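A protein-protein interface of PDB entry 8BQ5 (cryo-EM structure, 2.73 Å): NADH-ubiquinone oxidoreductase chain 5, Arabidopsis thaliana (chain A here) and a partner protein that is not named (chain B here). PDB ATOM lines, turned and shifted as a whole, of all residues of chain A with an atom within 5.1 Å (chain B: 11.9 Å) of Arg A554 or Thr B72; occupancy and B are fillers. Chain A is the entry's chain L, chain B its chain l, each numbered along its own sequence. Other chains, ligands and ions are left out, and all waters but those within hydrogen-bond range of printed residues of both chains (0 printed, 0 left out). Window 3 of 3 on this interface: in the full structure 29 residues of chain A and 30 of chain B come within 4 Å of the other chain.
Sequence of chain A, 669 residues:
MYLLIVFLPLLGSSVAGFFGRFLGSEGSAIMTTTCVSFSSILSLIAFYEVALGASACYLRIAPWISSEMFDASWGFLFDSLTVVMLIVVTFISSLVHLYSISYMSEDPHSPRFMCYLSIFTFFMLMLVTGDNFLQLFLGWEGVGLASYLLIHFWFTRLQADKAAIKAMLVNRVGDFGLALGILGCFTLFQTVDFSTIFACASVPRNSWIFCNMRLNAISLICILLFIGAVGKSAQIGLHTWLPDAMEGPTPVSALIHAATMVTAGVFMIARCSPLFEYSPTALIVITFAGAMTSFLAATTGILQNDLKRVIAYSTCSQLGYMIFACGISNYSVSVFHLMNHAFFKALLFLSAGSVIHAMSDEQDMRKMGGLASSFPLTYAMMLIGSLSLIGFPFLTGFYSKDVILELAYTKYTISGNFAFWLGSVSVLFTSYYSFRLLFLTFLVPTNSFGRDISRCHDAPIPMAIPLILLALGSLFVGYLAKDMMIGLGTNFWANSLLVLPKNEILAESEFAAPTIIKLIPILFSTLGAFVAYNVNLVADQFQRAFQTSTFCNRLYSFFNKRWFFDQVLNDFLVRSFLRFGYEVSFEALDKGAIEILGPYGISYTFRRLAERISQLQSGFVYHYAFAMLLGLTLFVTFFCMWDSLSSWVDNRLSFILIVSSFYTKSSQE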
ATOM      1  N   SER A 549     -11.780  20.637  43.590  1.00  0.00           N
ATOM      2  CA  SER A 549     -11.251  19.449  42.935  1.00  0.00           C
ATOM      3  C   SER A 549     -10.807  19.804  41.526  1.00  0.00           C
ATOM      4  O   SER A 549     -11.579  20.385  40.756  1.00  0.00           O
ATOM      5  CB  SER A 549     -12.294  18.331  42.893  1.00  0.00           C
ATOM      6  OG  SER A 549     -11.798  17.214  42.179  1.00  0.00           O
ATOM      7  N   THR A 550      -9.563  19.457  41.195  1.00  0.00           N
ATOM      8  CA  THR A 550      -9.060  19.722  39.853  1.00  0.00           C
ATOM      9  C   THR A 550      -9.837  18.927  38.809  1.00  0.00           C
ATOM     10  O   THR A 550     -10.156  19.450  37.736  1.00  0.00           O
ATOM     11  CB  THR A 550      -7.569  19.397  39.782  1.00  0.00           C
ATOM     12  OG1 THR A 550      -6.843  20.324  40.597  1.00  0.00           O
ATOM     13  CG2 THR A 550      -7.061  19.504  38.350  1.00  0.00           C
ATOM     14  N   PHE A 551     -10.159  17.666  39.112  1.00  0.00           N
ATOM     15  CA  PHE A 551     -10.866  16.830  38.148  1.00  0.00           C
ATOM     16  C   PHE A 551     -12.299  17.309  37.944  1.00  0.00           C
ATOM     17  O   PHE A 551     -12.789  17.352  36.810  1.00  0.00           O
ATOM     18  CB  PHE A 551     -10.846  15.371  38.605  1.00  0.00           C
ATOM     19  CG  PHE A 551     -11.422  14.413  37.600  1.00  0.00           C
ATOM     20  CD1 PHE A 551     -10.677  14.014  36.503  1.00  0.00           C
ATOM     21  CD2 PHE A 551     -12.705  13.916  37.748  1.00  0.00           C
ATOM     22  CE1 PHE A 551     -11.199  13.136  35.575  1.00  0.00           C
ATOM     23  CE2 PHE A 551     -13.232  13.037  36.821  1.00  0.00           C
ATOM     24  CZ  PHE A 551     -12.477  12.647  35.734  1.00  0.00           C
ATOM     25  N   CYS A 552     -12.986  17.669  39.029  1.00  0.00           N
ATOM     26  CA  CYS A 552     -14.343  18.189  38.903  1.00  0.00           C
ATOM     27  C   CYS A 552     -14.347  19.567  38.257  1.00  0.00           C
ATOM     28  O   CYS A 552     -15.284  19.915  37.529  1.00  0.00           O
ATOM     29  CB  CYS A 552     -15.020  18.233  40.273  1.00  0.00           C
ATOM     30  SG  CYS A 552     -15.806  16.681  40.757  1.00  0.00           S
ATOM     31  N   ASN A 553     -13.319  20.374  38.529  1.00  0.00           N
ATOM     32  CA  ASN A 553     -13.172  21.645  37.826  1.00  0.00           C
ATOM     33  C   ASN A 553     -12.932  21.422  36.341  1.00  0.00           C
ATOM     34  O   ASN A 553     -13.531  22.097  35.495  1.00  0.00           O
ATOM     35  CB  ASN A 553     -12.026  22.452  38.434  1.00  0.00           C
ATOM     36  CG  ASN A 553     -12.016  23.892  37.968  1.00  0.00           C
ATOM     37  OD1 ASN A 553     -11.282  24.253  37.049  1.00  0.00           O
ATOM     38  ND2 ASN A 553     -12.827  24.725  38.606  1.00  0.00           N
ATOM     39  N   ARG A 554     -12.060  20.471  36.003  1.00  0.00           N
ATOM     40  CA  ARG A 554     -11.746  20.210  34.603  1.00  0.00           C
ATOM     41  C   ARG A 554     -12.917  19.562  33.877  1.00  0.00           C
ATOM     42  O   ARG A 554     -13.117  19.792  32.680  1.00  0.00           O
ATOM     43  CB  ARG A 554     -10.504  19.332  34.503  1.00  0.00           C
ATOM     44  CG  ARG A 554      -9.218  20.078  34.756  1.00  0.00           C
ATOM     45  CD  ARG A 554      -8.573  20.439  33.441  1.00  0.00           C
ATOM     46  NE  ARG A 554      -7.682  21.589  33.547  1.00  0.00           N
ATOM     47  CZ  ARG A 554      -8.084  22.840  33.727  1.00  0.00           C
ATOM     48  NH1 ARG A 554      -9.368  23.150  33.808  1.00  0.00           N
ATOM     49  NH2 ARG A 554      -7.174  23.805  33.826  1.00  0.00           N
ATOM     50  N   LEU A 555     -13.690  18.735  34.581  1.00  0.00           N
ATOM     51  CA  LEU A 555     -14.850  18.104  33.962  1.00  0.00           C
ATOM     52  C   LEU A 555     -15.931  19.134  33.655  1.00  0.00           C
ATOM     53  O   LEU A 555     -16.636  19.027  32.645  1.00  0.00           O
ATOM     54  CB  LEU A 555     -15.380  16.991  34.868  1.00  0.00           C
ATOM     55  CG  LEU A 555     -16.136  15.852  34.186  1.00  0.00           C
ATOM     56  CD1 LEU A 555     -15.837  14.515  34.843  1.00  0.00           C
ATOM     57  CD2 LEU A 555     -17.614  16.143  34.246  1.00  0.00           C
ATOM     58  N   TYR A 556     -16.079  20.140  34.520  1.00  0.00           N
ATOM     59  CA  TYR A 556     -17.008  21.227  34.237  1.00  0.00           C
ATOM     60  C   TYR A 556     -16.561  22.020  33.014  1.00  0.00           C
ATOM     61  O   TYR A 556     -17.377  22.380  32.158  1.00  0.00           O
ATOM     62  CB  TYR A 556     -17.142  22.130  35.470  1.00  0.00           C
ATOM     63  CG  TYR A 556     -18.107  23.292  35.324  1.00  0.00           C
ATOM     64  CD1 TYR A 556     -19.317  23.302  36.007  1.00  0.00           C
ATOM     65  CD2 TYR A 556     -17.791  24.399  34.548  1.00  0.00           C
ATOM     66  CE1 TYR A 556     -20.195  24.361  35.888  1.00  0.00           C
ATOM     67  CE2 TYR A 556     -18.660  25.457  34.422  1.00  0.00           C
ATOM     68  CZ  TYR A 556     -19.859  25.436  35.093  1.00  0.00           C
ATOM     69  OH  TYR A 556     -20.718  26.500  34.966  1.00  0.00           O
ATOM     70  N   SER A 557     -15.260  22.305  32.916  1.00  0.00           N
ATOM     71  CA  SER A 557     -14.751  23.055  31.772  1.00  0.00           C
ATOM     72  C   SER A 557     -14.860  22.241  30.488  1.00  0.00           C
ATOM     73  O   SER A 557     -15.120  22.793  29.413  1.00  0.00           O
ATOM     74  CB  SER A 557     -13.304  23.481  32.024  1.00  0.00           C
ATOM     75  OG  SER A 557     -13.227  24.383  33.114  1.00  0.00           O
ATOM     76  N   PHE A 558     -14.663  20.924  30.583  1.00  0.00           N
ATOM     77  CA  PHE A 558     -14.778  20.057  29.414  1.00  0.00           C
ATOM     78  C   PHE A 558     -16.148  20.188  28.759  1.00  0.00           C
ATOM     79  O   PHE A 558     -16.255  20.429  27.552  1.00  0.00           O
ATOM     80  CB  PHE A 558     -14.523  18.605  29.824  1.00  0.00           C
ATOM     81  CG  PHE A 558     -14.558  17.633  28.680  1.00  0.00           C
ATOM     82  CD1 PHE A 558     -13.507  17.556  27.784  1.00  0.00           C
ATOM     83  CD2 PHE A 558     -15.644  16.791  28.504  1.00  0.00           C
ATOM     84  CE1 PHE A 558     -13.537  16.656  26.736  1.00  0.00           C
ATOM     85  CE2 PHE A 558     -15.681  15.892  27.457  1.00  0.00           C
ATOM     86  CZ  PHE A 558     -14.627  15.826  26.571  1.00  0.00           C
ATOM     87  N   LYS A 561     -17.031  23.968  27.638  1.00  0.00           N
ATOM     88  CA  LYS A 561     -16.268  24.408  26.476  1.00  0.00           C
ATOM     89  C   LYS A 561     -16.368  23.430  25.310  1.00  0.00           C
ATOM     90  O   LYS A 561     -15.430  23.321  24.514  1.00  0.00           O
ATOM     91  CB  LYS A 561     -14.806  24.637  26.855  1.00  0.00           C
ATOM     92  CG  LYS A 561     -14.457  26.093  27.092  1.00  0.00           C
ATOM     93  CD  LYS A 561     -13.639  26.261  28.356  1.00  0.00           C
ATOM     94  CE  LYS A 561     -12.200  26.609  28.021  1.00  0.00           C
ATOM     95  NZ  LYS A 561     -11.477  27.168  29.190  1.00  0.00           N
ATOM     96  N   PHE A 564     -13.744  20.718  24.228  1.00  0.00           N
ATOM     97  CA  PHE A 564     -12.547  21.318  23.636  1.00  0.00           C
ATOM     98  C   PHE A 564     -12.435  21.045  22.140  1.00  0.00           C
ATOM     99  O   PHE A 564     -11.330  20.942  21.610  1.00  0.00           O
ATOM    100  CB  PHE A 564     -11.266  20.850  24.334  1.00  0.00           C
ATOM    101  CG  PHE A 564     -11.310  20.953  25.826  1.00  0.00           C
ATOM    102  CD1 PHE A 564     -11.756  22.108  26.441  1.00  0.00           C
ATOM    103  CD2 PHE A 564     -10.891  19.897  26.614  1.00  0.00           C
ATOM    104  CE1 PHE A 564     -11.792  22.204  27.815  1.00  0.00           C
ATOM    105  CE2 PHE A 564     -10.923  19.987  27.987  1.00  0.00           C
ATOM    106  CZ  PHE A 564     -11.373  21.141  28.588  1.00  0.00           C
ATOM    107  N   ALA B  70     -10.481  28.849  25.437  1.00  0.00           N
ATOM    108  CA  ALA B  70      -9.098  28.508  25.121  1.00  0.00           C
ATOM    109  C   ALA B  70      -8.133  29.326  25.972  1.00  0.00           C
ATOM    110  O   ALA B  70      -7.093  29.773  25.489  1.00  0.00           O
ATOM    111  CB  ALA B  70      -8.822  28.730  23.642  1.00  0.00           C
ATOM    112  N   ASP B  71      -8.482  29.515  27.244  1.00  0.00           N
ATOM    113  CA  ASP B  71      -7.685  30.351  28.131  1.00  0.00           C
ATOM    114  C   ASP B  71      -7.286  29.592  29.392  1.00  0.00           C
ATOM    115  O   ASP B  71      -6.196  29.805  29.933  1.00  0.00           O
ATOM    116  CB  ASP B  71      -8.458  31.623  28.489  1.00  0.00           C
ATOM    117  CG  ASP B  71      -7.553  32.763  28.920  1.00  0.00           C
ATOM    118  OD1 ASP B  71      -6.592  32.520  29.677  1.00  0.00           O
ATOM    119  OD2 ASP B  71      -7.807  33.911  28.498  1.00  0.00           O
ATOM    120  N   THR B  72      -8.155  28.698  29.867  1.00  0.00           N
ATOM    121  CA  THR B  72      -7.905  27.984  31.111  1.00  0.00           C
ATOM    122  C   THR B  72      -7.318  26.592  30.922  1.00  0.00           C
ATOM    123  O   THR B  72      -6.785  26.034  31.885  1.00  0.00           O
ATOM    124  CB  THR B  72      -9.199  27.869  31.932  1.00  0.00           C
ATOM    125  OG1 THR B  72     -10.273  27.447  31.084  1.00  0.00           O
ATOM    126  CG2 THR B  72      -9.555  29.212  32.554  1.00  0.00           C
ATOM    127  N   VAL B  73      -7.386  26.028  29.720  1.00  0.00           N
ATOM    128  CA  VAL B  73      -6.884  24.686  29.443  1.00  0.00           C
ATOM    129  C   VAL B  73      -5.817  24.774  28.360  1.00  0.00           C
ATOM    130  O   VAL B  73      -5.991  25.475  27.356  1.00  0.00           O
ATOM    131  CB  VAL B  73      -8.034  23.746  29.028  1.00  0.00           C
ATOM    132  CG1 VAL B  73      -7.503  22.519  28.302  1.00  0.00           C
ATOM    133  CG2 VAL B  73      -8.854  23.339  30.248  1.00  0.00           C
ATOM    134  N   GLY B  74      -4.705  24.069  28.567  1.00  0.00           N
ATOM    135  CA  GLY B  74      -3.598  24.109  27.632  1.00  0.00           C
ATOM    136  C   GLY B  74      -3.893  23.384  26.329  1.00  0.00           C
ATOM    137  O   GLY B  74      -4.976  22.845  26.102  1.00  0.00           O
ATOM    138  N   LYS B  75      -2.886  23.370  25.451  1.00  0.00           N
ATOM    139  CA  LYS B  75      -3.088  22.868  24.094  1.00  0.00           C
ATOM    140  C   LYS B  75      -3.127  21.344  24.061  1.00  0.00           C
ATOM    141  O   LYS B  75      -4.135  20.745  23.668  1.00  0.00           O
ATOM    142  CB  LYS B  75      -1.992  23.395  23.166  1.00  0.00           C
ATOM    143  CG  LYS B  75      -1.792  22.553  21.914  1.00  0.00           C
ATOM    144  CD  LYS B  75      -0.429  22.778  21.290  1.00  0.00           C
ATOM    145  CE  LYS B  75      -0.439  23.982  20.366  1.00  0.00           C
ATOM    146  NZ  LYS B  75       0.578  23.856  19.286  1.00  0.00           N
ATOM    147  N   TYR B  76      -2.028  20.696  24.459  1.00  0.00           N
ATOM    148  CA  TYR B  76      -1.966  19.239  24.383  1.00  0.00           C
ATOM    149  C   TYR B  76      -2.873  18.587  25.413  1.00  0.00           C
ATOM    150  O   TYR B  76      -3.371  17.478  25.186  1.00  0.00           O
ATOM    151  CB  TYR B  76      -0.528  18.759  24.565  1.00  0.00           C
ATOM    152  CG  TYR B  76       0.361  19.054  23.384  1.00  0.00           C
ATOM    153  CD1 TYR B  76       0.332  18.254  22.252  1.00  0.00           C
ATOM    154  CD2 TYR B  76       1.227  20.138  23.399  1.00  0.00           C
ATOM    155  CE1 TYR B  76       1.142  18.522  21.168  1.00  0.00           C
ATOM    156  CE2 TYR B  76       2.041  20.415  22.321  1.00  0.00           C
ATOM    157  CZ  TYR B  76       1.994  19.605  21.207  1.00  0.00           C
ATOM    158  OH  TYR B  76       2.806  19.877  20.130  1.00  0.00           O
ATOM    159  N   GLU B  77      -3.083  19.248  26.550  1.00  0.00           N
ATOM    160  CA  GLU B  77      -4.022  18.737  27.541  1.00  0.00           C
ATOM    161  C   GLU B  77      -5.441  18.703  26.984  1.00  0.00           C
ATOM    162  O   GLU B  77      -6.196  17.757  27.236  1.00  0.00           O
ATOM    163  CB  GLU B  77      -3.952  19.591  28.804  1.00  0.00           C
ATOM    164  CG  GLU B  77      -4.970  19.217  29.854  1.00  0.00           C
ATOM    165  CD  GLU B  77      -5.511  20.432  30.562  1.00  0.00           C
ATOM    166  OE1 GLU B  77      -6.495  20.289  31.309  1.00  0.00           O
ATOM    167  OE2 GLU B  77      -4.948  21.530  30.373  1.00  0.00           O
ATOM    168  N   ALA B  78      -5.819  19.730  26.219  1.00  0.00           N
ATOM    169  CA  ALA B  78      -7.143  19.742  25.601  1.00  0.00           C
ATOM    170  C   ALA B  78      -7.303  18.585  24.626  1.00  0.00           C
ATOM    171  O   ALA B  78      -8.372  17.967  24.554  1.00  0.00           O
ATOM    172  CB  ALA B  78      -7.385  21.073  24.892  1.00  0.00           C
ATOM    173  N   LEU B  79      -6.256  18.285  23.857  1.00  0.00           N
ATOM    174  CA  LEU B  79      -6.306  17.141  22.954  1.00  0.00           C
ATOM    175  C   LEU B  79      -6.437  15.836  23.727  1.00  0.00           C
ATOM    176  O   LEU B  79      -7.146  14.918  23.297  1.00  0.00           O
ATOM    177  CB  LEU B  79      -5.063  17.118  22.066  1.00  0.00           C
ATOM    178  CG  LEU B  79      -4.826  15.838  21.263  1.00  0.00           C
ATOM    179  CD1 LEU B  79      -5.840  15.705  20.139  1.00  0.00           C
ATOM    180  CD2 LEU B  79      -3.412  15.810  20.714  1.00  0.00           C
ATOM    181  N   ALA B  80      -5.751  15.730  24.867  1.00  0.00           N
ATOM    182  CA  ALA B  80      -5.840  14.523  25.681  1.00  0.00           C
ATOM    183  C   ALA B  80      -7.257  14.314  26.201  1.00  0.00           C
ATOM    184  O   ALA B  80      -7.765  13.186  26.209  1.00  0.00           O
ATOM    185  CB  ALA B  80      -4.844  14.597  26.837  1.00  0.00           C
ATOM    186  N   TRP B  81      -7.906  15.390  26.647  1.00  0.00           N
ATOM    187  CA  TRP B  81      -9.287  15.286  27.112  1.00  0.00           C
ATOM    188  C   TRP B  81     -10.231  14.914  25.975  1.00  0.00           C
ATOM    189  O   TRP B  81     -11.126  14.078  26.145  1.00  0.00           O
ATOM    190  CB  TRP B  81      -9.718  16.601  27.762  1.00  0.00           C
ATOM    191  CG  TRP B  81      -9.415  16.664  29.219  1.00  0.00           C
ATOM    192  CD1 TRP B  81      -8.244  17.049  29.797  1.00  0.00           C
ATOM    193  CD2 TRP B  81     -10.299  16.321  30.292  1.00  0.00           C
ATOM    194  NE1 TRP B  81      -8.343  16.971  31.163  1.00  0.00           N
ATOM    195  CE2 TRP B  81      -9.596  16.526  31.493  1.00  0.00           C
ATOM    196  CE3 TRP B  81     -11.618  15.862  30.352  1.00  0.00           C
ATOM    197  CZ2 TRP B  81     -10.165  16.287  32.740  1.00  0.00           C
ATOM    198  CZ3 TRP B  81     -12.181  15.627  31.590  1.00  0.00           C
ATOM    199  CH2 TRP B  81     -11.457  15.841  32.767  1.00  0.00           C
ATOM    200  N   LEU B  82     -10.049  15.531  24.803  1.00  0.00           N
ATOM    201  CA  LEU B  82     -10.948  15.275  23.681  1.00  0.00           C
ATOM    202  C   LEU B  82     -10.801  13.851  23.162  1.00  0.00           C
ATOM    203  O   LEU B  82     -11.774  13.252  22.691  1.00  0.00           O
ATOM    204  CB  LEU B  82     -10.693  16.287  22.563  1.00  0.00           C
ATOM    205  CG  LEU B  82     -11.458  16.077  21.253  1.00  0.00           C
ATOM    206  CD1 LEU B  82     -12.954  16.217  21.470  1.00  0.00           C
ATOM    207  CD2 LEU B  82     -10.984  17.059  20.201  1.00  0.00           C
ATOM    208  N   GLY B  84     -10.151  11.328  25.073  1.00  0.00           N
ATOM    209  CA  GLY B  84     -10.923  10.544  26.021  1.00  0.00           C
ATOM    210  C   GLY B  84     -12.403  10.528  25.692  1.00  0.00           C
ATOM    211  O   GLY B  84     -13.060   9.490  25.795  1.00  0.00           O
ATOM    212  N   GLY B  85     -12.949  11.680  25.295  1.00  0.00           N
ATOM    213  CA  GLY B  85     -14.341  11.721  24.880  1.00  0.00           C
ATOM    214  C   GLY B  85     -14.595  10.915  23.623  1.00  0.00           C
ATOM    215  O   GLY B  85     -15.606  10.217  23.511  1.00  0.00           O
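The side-chain carboxylate of Glu B77 lies within hydrogen-bond range of the backbone NH of Gly B74 (3.1 Å).
Of the 15 printed residues of chain B, 6 touch a printed residue of chain A. Hydrophobic or aromatic side chains of chain B within 4 Å of the printed part of chain A: Val B73, Ala B78 and Trp B81. Printed residues of chain A that touch a printed residue of chain B: Phe A551, Arg A554, Phe A558, Lys A561 and Phe A564. Hydrophobic or aromatic side chains of chain A that line the printed part of chain B: Phe A551, Phe A558 and Phe A564. Among the printed residues, 11 pairs touch across the chains. Among the printed residues, Asp or Glu carboxylates within 4 Å of a Lys or Arg side-chain nitrogen of the other chain: Arg A554 with Glu B77 (2.8 Å).
Among the printed residues, merely in contact across the chains: Phe A551 with Trp B81 (3.9 Å), Arg A554 with Val B73 (3.6 Å), Arg A554 with Trp B81 (3.5 Å), Phe A558 with Trp B81 (3.6 Å), Lys A561 with Ala B70 (3.8 Å), Phe A564 with Val B73 (3.7 Å), Phe A564 with Ala B78 (3.8 Å) and Phe A564 with Trp B81 (3.6 Å).
No residue of chain B comes within 4 Å of Ser A549. Of the printed residues of chain B, Phe A551 touches Trp B81. No residue of chain B comes within 4 Å of Cys A552. No residue of chain B comes within 4 Å of Asn A553. Arg A554 touches just these residues of chain B: Thr B72, Val B73, Glu B77 and Trp B81. No residue of chain B comes within 4 Å of Leu A555. Of chain B, only Trp B81 comes within 4 Å of Phe A558. Printed residues of chain B within 4 Å of Lys A561: Ala B70 and Thr B72. Printed residues of chain B within 4 Å of Phe A564: Val B73, Ala B78 and Trp B81. Asp B71 touches none of the printed residues of chain A. Of the printed residues of chain A, Val B73 touches Arg A554 (3.6 Å) and Phe A564 (3.7 Å). Gly B74 touches none of the printed residues of chain A. Of the printed residues of chain A, Glu B77 touches Arg A554 (2.8 Å). Of the printed residues of chain A, Trp B81 touches Phe A551, Arg A554, Phe A558 and Phe A564.
O of Thr B72 lies within hydrogen-bond range of NH2 of Arg A554, at 3.0 Å. The side-chain carboxylate (OE1) of Glu B77 is in salt-bridge range of the guanidinium group (NE) of Arg A554. The side-chain amino group (NZ) of Lys A561 sits close to the side-chain hydroxyl (OG1) of Thr B72 (2.3 Å).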
